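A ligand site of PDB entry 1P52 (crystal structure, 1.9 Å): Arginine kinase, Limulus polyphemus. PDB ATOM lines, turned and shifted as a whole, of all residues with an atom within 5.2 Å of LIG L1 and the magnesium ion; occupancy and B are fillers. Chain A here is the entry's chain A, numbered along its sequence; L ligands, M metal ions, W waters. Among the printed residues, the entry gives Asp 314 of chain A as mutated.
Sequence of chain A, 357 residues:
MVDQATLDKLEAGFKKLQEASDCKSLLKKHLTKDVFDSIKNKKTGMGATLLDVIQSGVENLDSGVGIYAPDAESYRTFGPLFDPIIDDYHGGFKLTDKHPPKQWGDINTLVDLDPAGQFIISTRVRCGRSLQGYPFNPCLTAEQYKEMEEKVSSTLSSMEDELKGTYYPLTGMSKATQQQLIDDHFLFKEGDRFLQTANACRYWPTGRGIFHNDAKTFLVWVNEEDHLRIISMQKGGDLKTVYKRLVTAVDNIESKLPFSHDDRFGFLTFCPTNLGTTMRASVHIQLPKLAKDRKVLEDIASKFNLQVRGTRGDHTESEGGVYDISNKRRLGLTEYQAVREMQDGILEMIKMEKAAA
N of Arg 309 lies within hydrogen-bond range of O of Asp 324, at 2.8 Å.
The backbone NH (N) of His 284 sits at hydrogen-bond distance from the backbone carbonyl oxygen (O) of Ser 122, at 2.9 Å.
The side-chain carboxylate of Asp 324 lies within salt-bridge range of the guanidinium group of Arg 280.
OE1 of Glu 225 is in salt-bridge range of NH2 of Arg 229, 3.2 Å away.
The guanidinium group (NE) of Arg 124 lies within hydrogen-bond range of the side-chain sulfur (SD) of Met 233 (3.8 Å).
The side-chain carboxylate of Asp 314 lies within salt-bridge range of the guanidinium group of Arg 309 (3.9 Å).
The backbone carbonyl oxygen (O) of Arg 229 sits at hydrogen-bond distance from the backbone NH (N) of Trp 221, at 2.9 Å.
O of Thr 311 sits close to NE2 of His 284.
No residue comes within 4 Å of the magnesium ion.
The nearest printed residue that does not touch the magnesium ion is Arg 229 (4.2 Å).
The guanidinium group (NH1) of Arg 124 lies within salt-bridge range of an oxygen (O2) of LIG L1, 3.0 Å away.
The guanidinium group of Arg 229 lies within salt-bridge range of an oxygen (O3) of LIG L1.
NH1 of Arg 309 lies within salt-bridge range of O5 of LIG L1 (2.8 Å).
O of Ser 282 is in hydrogen-bond range of N3 of LIG L1.
O of Thr 311 is in hydrogen-bond range of O10 of LIG L1 (2.8 Å).
A nitrogen (N2) of LIG L1 sits at hydrogen-bond distance from the side-chain hydroxyl (OG) of Ser 282, 2.7 Å away.
The side-chain carboxylate (OD2) of Asp 314 is in salt-bridge range of a nitrogen (N2) of LG3 L3 (2.8 Å).
N4 of LIG L1 lies within hydrogen-bond range of OG of Ser 122, at 2.7 Å.
N3 of LIG L1 is in hydrogen-bond range of O of Ser 122 (3.4 Å).
OE2 of Glu 225 is in salt-bridge range of N4 of LG3 L3.
A ring nitrogen (ND1) of His 185 is in hydrogen-bond range of an oxygen (O10) of LIG L1, at 3.0 Å.
NE of Arg 280 lies within salt-bridge range of O3 of LIG L1, 2.8 Å away.
NH1 of Arg 126 is in salt-bridge range of O3 of LIG L1 (2.5 Å).
N of Asp 314 sits at hydrogen-bond distance from O5 of LIG L1, at 3.0 Å.
The magnesium ion is bound by an oxygen (O1) of LIG L1 (2.0 Å).
The magnesium ion is bound by an oxygen (O4) of LIG L1 (2.0 Å).
The magnesium ion is bound by water W8, at 2.1 Å.
The magnesium ion is bound by an oxygen (O1) of LG2 L2, 2.1 Å away.
The magnesium ion is bound by water W1 (2.1 Å).
Water W2 is bound to the magnesium ion (2.2 Å).
The backbone NH of His 284 sits close to a nitrogen (N3) of LIG L1, at 3.4 Å.
Residues that only touch LIG L1: Gly 313, Val 283, Asp 324, Trp 221, Arg 312 and Met 233.
Hydrophobic or aromatic side chains within 4 Å of LIG L1: His 185, Trp 221, Met 233 and His 284.
Within 4 Å of LIG L1: Ser 122, Arg 124, Arg 126, His 185, Trp 221, Arg 229, Met 233, Arg 280, Ser 282, Val 283, His 284, Arg 309, Thr 311, Arg 312, Gly 313, Asp 314 and Asp 324.
The nearest printed residue that does not touch LIG L1 is Thr 123 (4.03 Å).
Water W2 lies within hydrogen-bond range of the side-chain carboxylate (OE2) of Glu 225 (2.8 Å), the side-chain carboxylate (OE1) of Glu 224 (2.9 Å) and the guanidinium group (NH1) of Arg 229 (3.4 Å).
Water W4 bridges an oxygen (O2) of LIG L1 (2.7 Å) and the guanidinium group of Arg 229 (3.0 Å).
Water W7 bridges the backbone carbonyl oxygen (O) of Leu 187 (2.7 Å) and an oxygen (O9) of LIG L1 (2.8 Å).
Water W5 lies within hydrogen-bond range of O of Ile 182 (2.6 Å), O9 of LIG L1 (2.8 Å) and ND1 of His 185 (2.9 Å).
Water W6 lies within hydrogen-bond range of OD2 of Asp 324 (2.6 Å), NE2 of His 284 (2.9 Å), O10 of LIG L1 (3.0 Å), O of Thr 311 (3.2 Å) and N of Gly 313 (3.2 Å).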
ATOM      1  N   SER A 122     -20.239  18.169   5.601  1.00  0.00           N
ATOM      2  CA  SER A 122     -19.603  19.288   6.281  1.00  0.00           C
ATOM      3  C   SER A 122     -18.186  18.951   6.765  1.00  0.00           C
ATOM      4  O   SER A 122     -17.848  17.779   6.968  1.00  0.00           O
ATOM      5  CB  SER A 122     -20.453  19.743   7.468  1.00  0.00           C
ATOM      6  OG  SER A 122     -20.692  18.671   8.380  1.00  0.00           O
ATOM      7  N   THR A 123     -17.388  19.996   6.959  1.00  0.00           N
ATOM      8  CA  THR A 123     -16.008  19.844   7.381  1.00  0.00           C
ATOM      9  C   THR A 123     -15.779  20.697   8.620  1.00  0.00           C
ATOM     10  O   THR A 123     -16.280  21.815   8.720  1.00  0.00           O
ATOM     11  CB  THR A 123     -15.055  20.287   6.245  1.00  0.00           C
ATOM     12  OG1 THR A 123     -15.301  19.463   5.095  1.00  0.00           O
ATOM     13  CG2 THR A 123     -13.586  20.146   6.658  1.00  0.00           C
ATOM     14  N   ARG A 124     -15.016  20.144   9.559  1.00  0.00           N
ATOM     15  CA  ARG A 124     -14.758  20.839  10.824  1.00  0.00           C
ATOM     16  C   ARG A 124     -13.361  20.555  11.319  1.00  0.00           C
ATOM     17  O   ARG A 124     -12.851  19.452  11.136  1.00  0.00           O
ATOM     18  CB  ARG A 124     -15.774  20.339  11.855  1.00  0.00           C
ATOM     19  CG  ARG A 124     -15.630  20.824  13.307  1.00  0.00           C
ATOM     20  CD  ARG A 124     -16.837  20.231  14.036  1.00  0.00           C
ATOM     21  NE  ARG A 124     -17.026  20.600  15.440  1.00  0.00           N
ATOM     22  CZ  ARG A 124     -16.425  20.000  16.466  1.00  0.00           C
ATOM     23  NH1 ARG A 124     -15.566  19.013  16.254  1.00  0.00           N
ATOM     24  NH2 ARG A 124     -16.755  20.323  17.714  1.00  0.00           N
ATOM     25  N   ARG A 126     -11.019  21.423  14.888  1.00  0.00           N
ATOM     26  CA  ARG A 126     -10.991  22.027  16.213  1.00  0.00           C
ATOM     27  C   ARG A 126      -9.685  21.767  16.914  1.00  0.00           C
ATOM     28  O   ARG A 126      -8.967  20.822  16.568  1.00  0.00           O
ATOM     29  CB  ARG A 126     -12.134  21.503  17.114  1.00  0.00           C
ATOM     30  CG  ARG A 126     -12.168  19.987  17.415  1.00  0.00           C
ATOM     31  CD  ARG A 126     -11.207  19.540  18.545  1.00  0.00           C
ATOM     32  NE  ARG A 126     -11.592  18.222  19.082  1.00  0.00           N
ATOM     33  CZ  ARG A 126     -10.788  17.395  19.742  1.00  0.00           C
ATOM     34  NH1 ARG A 126     -11.253  16.229  20.183  1.00  0.00           N
ATOM     35  NH2 ARG A 126      -9.508  17.711  19.960  1.00  0.00           N
ATOM     36  N   ILE A 182     -27.170  21.838  19.829  1.00  0.00           N
ATOM     37  CA  ILE A 182     -26.552  20.519  19.894  1.00  0.00           C
ATOM     38  C   ILE A 182     -26.942  19.733  18.647  1.00  0.00           C
ATOM     39  O   ILE A 182     -26.084  19.162  17.962  1.00  0.00           O
ATOM     40  CB  ILE A 182     -27.013  19.738  21.150  1.00  0.00           C
ATOM     41  CG1 ILE A 182     -26.437  20.405  22.413  1.00  0.00           C
ATOM     42  CG2 ILE A 182     -26.569  18.291  21.043  1.00  0.00           C
ATOM     43  CD1 ILE A 182     -26.975  19.798  23.692  1.00  0.00           C
ATOM     44  N   HIS A 185     -25.144  20.355  15.608  1.00  0.00           N
ATOM     45  CA  HIS A 185     -23.729  19.956  15.716  1.00  0.00           C
ATOM     46  C   HIS A 185     -22.790  21.092  16.106  1.00  0.00           C
ATOM     47  O   HIS A 185     -21.580  21.026  15.846  1.00  0.00           O
ATOM     48  CB  HIS A 185     -23.256  19.340  14.382  1.00  0.00           C
ATOM     49  CG  HIS A 185     -24.132  18.234  13.905  1.00  0.00           C
ATOM     50  ND1 HIS A 185     -24.433  17.138  14.686  1.00  0.00           N
ATOM     51  CD2 HIS A 185     -24.843  18.090  12.765  1.00  0.00           C
ATOM     52  CE1 HIS A 185     -25.294  16.367  14.036  1.00  0.00           C
ATOM     53  NE2 HIS A 185     -25.565  16.922  12.872  1.00  0.00           N
ATOM     54  N   PHE A 186     -23.332  22.130  16.734  1.00  0.00           N
ATOM     55  CA  PHE A 186     -22.520  23.266  17.126  1.00  0.00           C
ATOM     56  C   PHE A 186     -22.073  23.233  18.586  1.00  0.00           C
ATOM     57  O   PHE A 186     -20.915  23.505  18.895  1.00  0.00           O
ATOM     58  CB  PHE A 186     -23.307  24.564  16.901  1.00  0.00           C
ATOM     59  CG  PHE A 186     -23.644  24.835  15.461  1.00  0.00           C
ATOM     60  CD1 PHE A 186     -24.957  25.104  15.086  1.00  0.00           C
ATOM     61  CD2 PHE A 186     -22.658  24.844  14.487  1.00  0.00           C
ATOM     62  CE1 PHE A 186     -25.277  25.374  13.749  1.00  0.00           C
ATOM     63  CE2 PHE A 186     -22.969  25.112  13.153  1.00  0.00           C
ATOM     64  CZ  PHE A 186     -24.277  25.382  12.796  1.00  0.00           C
ATOM     65  N   LEU A 187     -23.001  22.898  19.464  1.00  0.00           N
ATOM     66  CA  LEU A 187     -22.751  22.865  20.909  1.00  0.00           C
ATOM     67  C   LEU A 187     -22.486  21.486  21.485  1.00  0.00           C
ATOM     68  O   LEU A 187     -23.073  20.494  21.063  1.00  0.00           O
ATOM     69  CB  LEU A 187     -23.959  23.478  21.636  1.00  0.00           C
ATOM     70  CG  LEU A 187     -24.016  23.413  23.162  1.00  0.00           C
ATOM     71  CD1 LEU A 187     -22.892  24.249  23.744  1.00  0.00           C
ATOM     72  CD2 LEU A 187     -25.374  23.925  23.654  1.00  0.00           C
ATOM     73  N   TRP A 221     -16.073  26.586  22.575  1.00  0.00           N
ATOM     74  CA  TRP A 221     -16.732  25.947  23.704  1.00  0.00           C
ATOM     75  C   TRP A 221     -15.968  26.350  24.969  1.00  0.00           C
ATOM     76  O   TRP A 221     -14.740  26.280  24.993  1.00  0.00           O
ATOM     77  CB  TRP A 221     -16.673  24.415  23.611  1.00  0.00           C
ATOM     78  CG  TRP A 221     -17.505  23.776  22.544  1.00  0.00           C
ATOM     79  CD1 TRP A 221     -18.411  24.375  21.724  1.00  0.00           C
ATOM     80  CD2 TRP A 221     -17.509  22.376  22.206  1.00  0.00           C
ATOM     81  NE1 TRP A 221     -18.979  23.431  20.891  1.00  0.00           N
ATOM     82  CE2 TRP A 221     -18.448  22.200  21.165  1.00  0.00           C
ATOM     83  CE3 TRP A 221     -16.816  21.256  22.687  1.00  0.00           C
ATOM     84  CZ2 TRP A 221     -18.709  20.948  20.596  1.00  0.00           C
ATOM     85  CZ3 TRP A 221     -17.079  20.012  22.124  1.00  0.00           C
ATOM     86  CH2 TRP A 221     -18.017  19.872  21.088  1.00  0.00           C
ATOM     87  N   GLU A 224     -16.161  22.664  28.743  1.00  0.00           N
ATOM     88  CA  GLU A 224     -16.738  21.342  28.608  1.00  0.00           C
ATOM     89  C   GLU A 224     -15.573  20.421  29.002  1.00  0.00           C
ATOM     90  O   GLU A 224     -15.050  20.520  30.121  1.00  0.00           O
ATOM     91  CB  GLU A 224     -17.170  21.054  27.180  1.00  0.00           C
ATOM     92  CG  GLU A 224     -17.915  19.712  27.095  1.00  0.00           C
ATOM     93  CD  GLU A 224     -17.414  18.822  25.980  1.00  0.00           C
ATOM     94  OE1 GLU A 224     -16.228  18.956  25.593  1.00  0.00           O
ATOM     95  OE2 GLU A 224     -18.205  17.963  25.505  1.00  0.00           O
ATOM     96  N   GLU A 225     -15.130  19.552  28.090  1.00  0.00           N
ATOM     97  CA  GLU A 225     -14.059  18.607  28.410  1.00  0.00           C
ATOM     98  C   GLU A 225     -12.735  19.302  28.715  1.00  0.00           C
ATOM     99  O   GLU A 225     -12.019  18.925  29.649  1.00  0.00           O
ATOM    100  CB  GLU A 225     -13.893  17.589  27.278  1.00  0.00           C
ATOM    101  CG  GLU A 225     -12.709  16.639  27.487  1.00  0.00           C
ATOM    102  CD  GLU A 225     -12.668  15.534  26.449  1.00  0.00           C
ATOM    103  OE1 GLU A 225     -11.551  15.061  26.142  1.00  0.00           O
ATOM    104  OE2 GLU A 225     -13.745  15.134  25.964  1.00  0.00           O
ATOM    105  N   ARG A 229     -12.329  24.885  23.541  1.00  0.00           N
ATOM    106  CA  ARG A 229     -12.278  24.094  22.308  1.00  0.00           C
ATOM    107  C   ARG A 229     -12.554  25.185  21.265  1.00  0.00           C
ATOM    108  O   ARG A 229     -13.601  25.854  21.327  1.00  0.00           O
ATOM    109  CB  ARG A 229     -13.341  22.981  22.249  1.00  0.00           C
ATOM    110  CG  ARG A 229     -13.080  21.753  23.152  1.00  0.00           C
ATOM    111  CD  ARG A 229     -11.740  21.024  22.812  1.00  0.00           C
ATOM    112  NE  ARG A 229     -11.534  19.802  23.598  1.00  0.00           N
ATOM    113  CZ  ARG A 229     -12.182  18.655  23.405  1.00  0.00           C
ATOM    114  NH1 ARG A 229     -13.077  18.557  22.438  1.00  0.00           N
ATOM    115  NH2 ARG A 229     -11.922  17.581  24.163  1.00  0.00           N
ATOM    116  N   MET A 233     -15.899  25.478  11.321  1.00  0.00           N
ATOM    117  CA  MET A 233     -16.688  24.507  10.567  1.00  0.00           C
ATOM    118  C   MET A 233     -17.687  25.158   9.627  1.00  0.00           C
ATOM    119  O   MET A 233     -18.071  26.318   9.800  1.00  0.00           O
ATOM    120  CB  MET A 233     -17.445  23.575  11.537  1.00  0.00           C
ATOM    121  CG  MET A 233     -18.527  24.260  12.380  1.00  0.00           C
ATOM    122  SD  MET A 233     -19.156  23.235  13.756  1.00  0.00           S
ATOM    123  CE  MET A 233     -20.376  22.170  12.904  1.00  0.00           C
ATOM    124  N   ARG A 280      -8.469  17.826  15.918  1.00  0.00           N
ATOM    125  CA  ARG A 280      -9.319  16.782  15.353  1.00  0.00           C
ATOM    126  C   ARG A 280      -9.958  17.424  14.138  1.00  0.00           C
ATOM    127  O   ARG A 280     -10.802  18.331  14.258  1.00  0.00           O
ATOM    128  CB  ARG A 280     -10.387  16.307  16.356  1.00  0.00           C
ATOM    129  CG  ARG A 280     -11.240  15.109  15.822  1.00  0.00           C
ATOM    130  CD  ARG A 280     -12.038  14.456  16.951  1.00  0.00           C
ATOM    131  NE  ARG A 280     -13.446  14.842  16.974  1.00  0.00           N
ATOM    132  CZ  ARG A 280     -14.336  14.469  16.047  1.00  0.00           C
ATOM    133  NH1 ARG A 280     -13.955  13.707  15.034  1.00  0.00           N
ATOM    134  NH2 ARG A 280     -15.609  14.832  16.163  1.00  0.00           N
ATOM    135  N   SER A 282     -12.250  16.826  10.954  1.00  0.00           N
ATOM    136  CA  SER A 282     -13.255  15.849  10.577  1.00  0.00           C
ATOM    137  C   SER A 282     -14.195  16.267   9.472  1.00  0.00           C
ATOM    138  O   SER A 282     -14.300  17.438   9.116  1.00  0.00           O
ATOM    139  CB  SER A 282     -14.127  15.509  11.782  1.00  0.00           C
ATOM    140  OG  SER A 282     -15.027  16.590  12.045  1.00  0.00           O
ATOM    141  N   VAL A 283     -14.894  15.276   8.975  1.00  0.00           N
ATOM    142  CA  VAL A 283     -15.913  15.476   7.980  1.00  0.00           C
ATOM    143  C   VAL A 283     -17.116  14.630   8.363  1.00  0.00           C
ATOM    144  O   VAL A 283     -16.992  13.601   9.033  1.00  0.00           O
ATOM    145  CB  VAL A 283     -15.480  15.036   6.561  1.00  0.00           C
ATOM    146  CG1 VAL A 283     -14.372  15.947   6.042  1.00  0.00           C
ATOM    147  CG2 VAL A 283     -15.038  13.569   6.575  1.00  0.00           C
ATOM    148  N   HIS A 284     -18.295  15.105   7.989  1.00  0.00           N
ATOM    149  CA  HIS A 284     -19.499  14.324   8.177  1.00  0.00           C
ATOM    150  C   HIS A 284     -19.626  13.845   6.738  1.00  0.00           C
ATOM    151  O   HIS A 284     -19.723  14.668   5.814  1.00  0.00           O
ATOM    152  CB  HIS A 284     -20.666  15.177   8.629  1.00  0.00           C
ATOM    153  CG  HIS A 284     -20.885  15.141  10.112  1.00  0.00           C
ATOM    154  ND1 HIS A 284     -21.992  15.691  10.714  1.00  0.00           N
ATOM    155  CD2 HIS A 284     -20.163  14.567  11.100  1.00  0.00           C
ATOM    156  CE1 HIS A 284     -21.943  15.463  12.016  1.00  0.00           C
ATOM    157  NE2 HIS A 284     -20.839  14.789  12.280  1.00  0.00           N
ATOM    158  N   ARG A 309     -16.791   7.919  14.054  1.00  0.00           N
ATOM    159  CA  ARG A 309     -17.705   8.190  15.165  1.00  0.00           C
ATOM    160  C   ARG A 309     -19.092   8.353  14.582  1.00  0.00           C
ATOM    161  O   ARG A 309     -19.245   8.477  13.369  1.00  0.00           O
ATOM    162  CB  ARG A 309     -17.332   9.498  15.885  1.00  0.00           C
ATOM    163  CG  ARG A 309     -15.970   9.484  16.518  1.00  0.00           C
ATOM    164  CD  ARG A 309     -15.638  10.837  17.123  1.00  0.00           C
ATOM    165  NE  ARG A 309     -14.327  10.759  17.761  1.00  0.00           N
ATOM    166  CZ  ARG A 309     -13.915  11.593  18.711  1.00  0.00           C
ATOM    167  NH1 ARG A 309     -14.707  12.572  19.126  1.00  0.00           N
ATOM    168  NH2 ARG A 309     -12.723  11.400  19.268  1.00  0.00           N
ATOM    169  N   THR A 311     -22.939  10.216  14.134  1.00  0.00           N
ATOM    170  CA  THR A 311     -23.317  11.570  13.726  1.00  0.00           C
ATOM    171  C   THR A 311     -23.322  12.618  14.827  1.00  0.00           C
ATOM    172  O   THR A 311     -23.086  13.793  14.562  1.00  0.00           O
ATOM    173  CB  THR A 311     -24.700  11.569  13.057  1.00  0.00           C
ATOM    174  OG1 THR A 311     -24.839  10.401  12.250  1.00  0.00           O
ATOM    175  CG2 THR A 311     -24.851  12.801  12.176  1.00  0.00           C
ATOM    176  N   ARG A 312     -23.584  12.191  16.059  1.00  0.00           N
ATOM    177  CA  ARG A 312     -23.637  13.124  17.179  1.00  0.00           C
ATOM    178  C   ARG A 312     -22.359  13.181  17.979  1.00  0.00           C
ATOM    179  O   ARG A 312     -22.316  13.808  19.051  1.00  0.00           O
ATOM    180  CB  ARG A 312     -24.817  12.756  18.103  1.00  0.00           C
ATOM    181  CG  ARG A 312     -26.192  13.094  17.498  1.00  0.00           C
ATOM    182  CD  ARG A 312     -27.337  12.455  18.283  1.00  0.00           C
ATOM    183  NE  ARG A 312     -28.657  12.897  17.820  1.00  0.00           N
ATOM    184  CZ  ARG A 312     -29.198  14.076  18.111  1.00  0.00           C
ATOM    185  NH1 ARG A 312     -28.545  14.955  18.867  1.00  0.00           N
ATOM    186  NH2 ARG A 312     -30.399  14.390  17.642  1.00  0.00           N
ATOM    187  N   GLY A 313     -21.322  12.516  17.455  1.00  0.00           N
ATOM    188  CA  GLY A 313     -20.013  12.494  18.087  1.00  0.00           C
ATOM    189  C   GLY A 313     -19.621  11.202  18.778  1.00  0.00           C
ATOM    190  O   GLY A 313     -20.159  10.129  18.501  1.00  0.00           O
ATOM    191  N   ASP A 314     -18.631  11.332  19.660  1.00  0.00           N
ATOM    192  CA  ASP A 314     -18.085  10.284  20.520  1.00  0.00           C
ATOM    193  C   ASP A 314     -19.162   9.288  20.991  1.00  0.00           C
ATOM    194  O   ASP A 314     -20.178   9.703  21.542  1.00  0.00           O
ATOM    195  CB  ASP A 314     -17.522  10.986  21.767  1.00  0.00           C
ATOM    196  CG  ASP A 314     -16.145  10.526  22.153  1.00  0.00           C
ATOM    197  OD1 ASP A 314     -15.606   9.588  21.528  1.00  0.00           O
ATOM    198  OD2 ASP A 314     -15.615  11.147  23.106  1.00  0.00           O
ATOM    199  N   ASP A 324     -18.855  10.456  11.083  1.00  0.00           N
ATOM    200  CA  ASP A 324     -17.888  11.469  11.487  1.00  0.00           C
ATOM    201  C   ASP A 324     -16.545  10.723  11.316  1.00  0.00           C
ATOM    202  O   ASP A 324     -16.271   9.773  12.035  1.00  0.00           O
ATOM    203  CB  ASP A 324     -18.149  11.815  12.968  1.00  0.00           C
ATOM    204  CG  ASP A 324     -17.068  12.710  13.596  1.00  0.00           C
ATOM    205  OD1 ASP A 324     -15.898  12.656  13.149  1.00  0.00           O
ATOM    206  OD2 ASP A 324     -17.385  13.426  14.567  1.00  0.00           O
HETATM  207  P1  LIG L   1     -14.963  16.934  19.696  1.00  0.00           P
HETATM  208  O1  LIG L   1     -15.253  17.012  21.165  1.00  0.00           O
HETATM  209  O2  LIG L   1     -15.067  18.280  19.104  1.00  0.00           O
HETATM  210  O3  LIG L   1     -13.633  16.315  19.379  1.00  0.00           O
HETATM  211  P2  LIG L   1     -17.256  15.100  19.419  1.00  0.00           P
HETATM  212  O4  LIG L   1     -17.400  15.077  20.903  1.00  0.00           O
HETATM  213  O5  LIG L   1     -17.249  13.796  18.737  1.00  0.00           O
HETATM  214  O6  LIG L   1     -15.997  15.997  18.953  1.00  0.00           O
HETATM  215  O7  LIG L   1     -18.474  15.913  18.726  1.00  0.00           O
HETATM  216  C1  LIG L   1     -18.915  17.165  19.208  1.00  0.00           C
HETATM  217  C2  LIG L   1     -19.824  17.784  18.152  1.00  0.00           C
HETATM  218  O8  LIG L   1     -19.118  18.127  16.936  1.00  0.00           O
HETATM  219  C3  LIG L   1     -20.950  16.852  17.737  1.00  0.00           C
HETATM  220  O9  LIG L   1     -22.153  17.639  17.697  1.00  0.00           O
HETATM  221  C4  LIG L   1     -20.607  16.409  16.333  1.00  0.00           C
HETATM  222  O10 LIG L   1     -21.757  16.052  15.518  1.00  0.00           O
HETATM  223  C5  LIG L   1     -19.863  17.631  15.808  1.00  0.00           C
HETATM  224  N1  LIG L   1     -19.030  17.339  14.590  1.00  0.00           N
HETATM  225  C6  LIG L   1     -17.829  16.736  14.497  1.00  0.00           C
HETATM  226  N2  LIG L   1     -17.410  16.744  13.227  1.00  0.00           N
HETATM  227  C7  LIG L   1     -18.358  17.385  12.539  1.00  0.00           C
HETATM  228  C8  LIG L   1     -18.302  17.754  11.183  1.00  0.00           C
HETATM  229  N3  LIG L   1     -17.343  17.388  10.315  1.00  0.00           N
HETATM  230  N4  LIG L   1     -19.370  18.454  10.732  1.00  0.00           N
HETATM  231  C9  LIG L   1     -20.369  18.786  11.552  1.00  0.00           C
HETATM  232  N5  LIG L   1     -20.401  18.467  12.851  1.00  0.00           N
HETATM  233  C10 LIG L   1     -19.390  17.743  13.367  1.00  0.00           C
HETATM  234  N1  LG2 L   2     -13.343  14.481  21.856  1.00  0.00           N
HETATM  235  O1  LG2 L   2     -14.832  14.432  21.757  1.00  0.00           O
HETATM  236  O2  LG2 L   2     -12.441  13.558  21.105  1.00  0.00           O
HETATM  237  O3  LG2 L   2     -12.724  15.372  22.832  1.00  0.00           O
HETATM  238  N1  LG3 L   3     -13.061   8.286  27.830  1.00  0.00           N
HETATM  239  C1  LG3 L   3     -13.723   7.838  26.597  1.00  0.00           C
HETATM  240  C2  LG3 L   3     -13.503   8.862  25.481  1.00  0.00           C
HETATM  241  C3  LG3 L   3     -12.041   9.147  25.134  1.00  0.00           C
HETATM  242  C4  LG3 L   3     -11.899   9.863  23.770  1.00  0.00           C
HETATM  243  N2  LG3 L   3     -12.833  10.987  23.679  1.00  0.00           N
HETATM  244  C5  LG3 L   3     -12.673  12.159  24.275  1.00  0.00           C
HETATM  245  N3  LG3 L   3     -11.594  12.413  25.024  1.00  0.00           N
HETATM  246  N4  LG3 L   3     -13.624  13.083  24.155  1.00  0.00           N
HETATM  247  C6  LG3 L   3     -13.224   6.467  26.133  1.00  0.00           C
HETATM  248  O1  LG3 L   3     -12.127   6.051  26.510  1.00  0.00           O
HETATM  249 MG    MG M   1     -16.276  15.822  22.410  1.00  0.00          MG
HETATM  250  O   HOH W   1     -17.932  16.999  23.068  1.00  0.00           O
HETATM  251  O   HOH W   2     -15.260  16.650  24.127  1.00  0.00           O
HETATM  252  O   HOH W   3     -19.718  14.267  22.271  1.00  0.00           O
HETATM  253  O   HOH W   4     -14.183  20.441  20.400  1.00  0.00           O
HETATM  254  O   HOH W   5     -24.885  16.855  17.572  1.00  0.00           O
HETATM  255  O   HOH W   6     -19.939  13.718  14.807  1.00  0.00           O
HETATM  256  O   HOH W   7     -22.641  17.932  20.404  1.00  0.00           O
HETATM  257  O   HOH W   8     -16.960  14.288  23.665  1.00  0.00           O
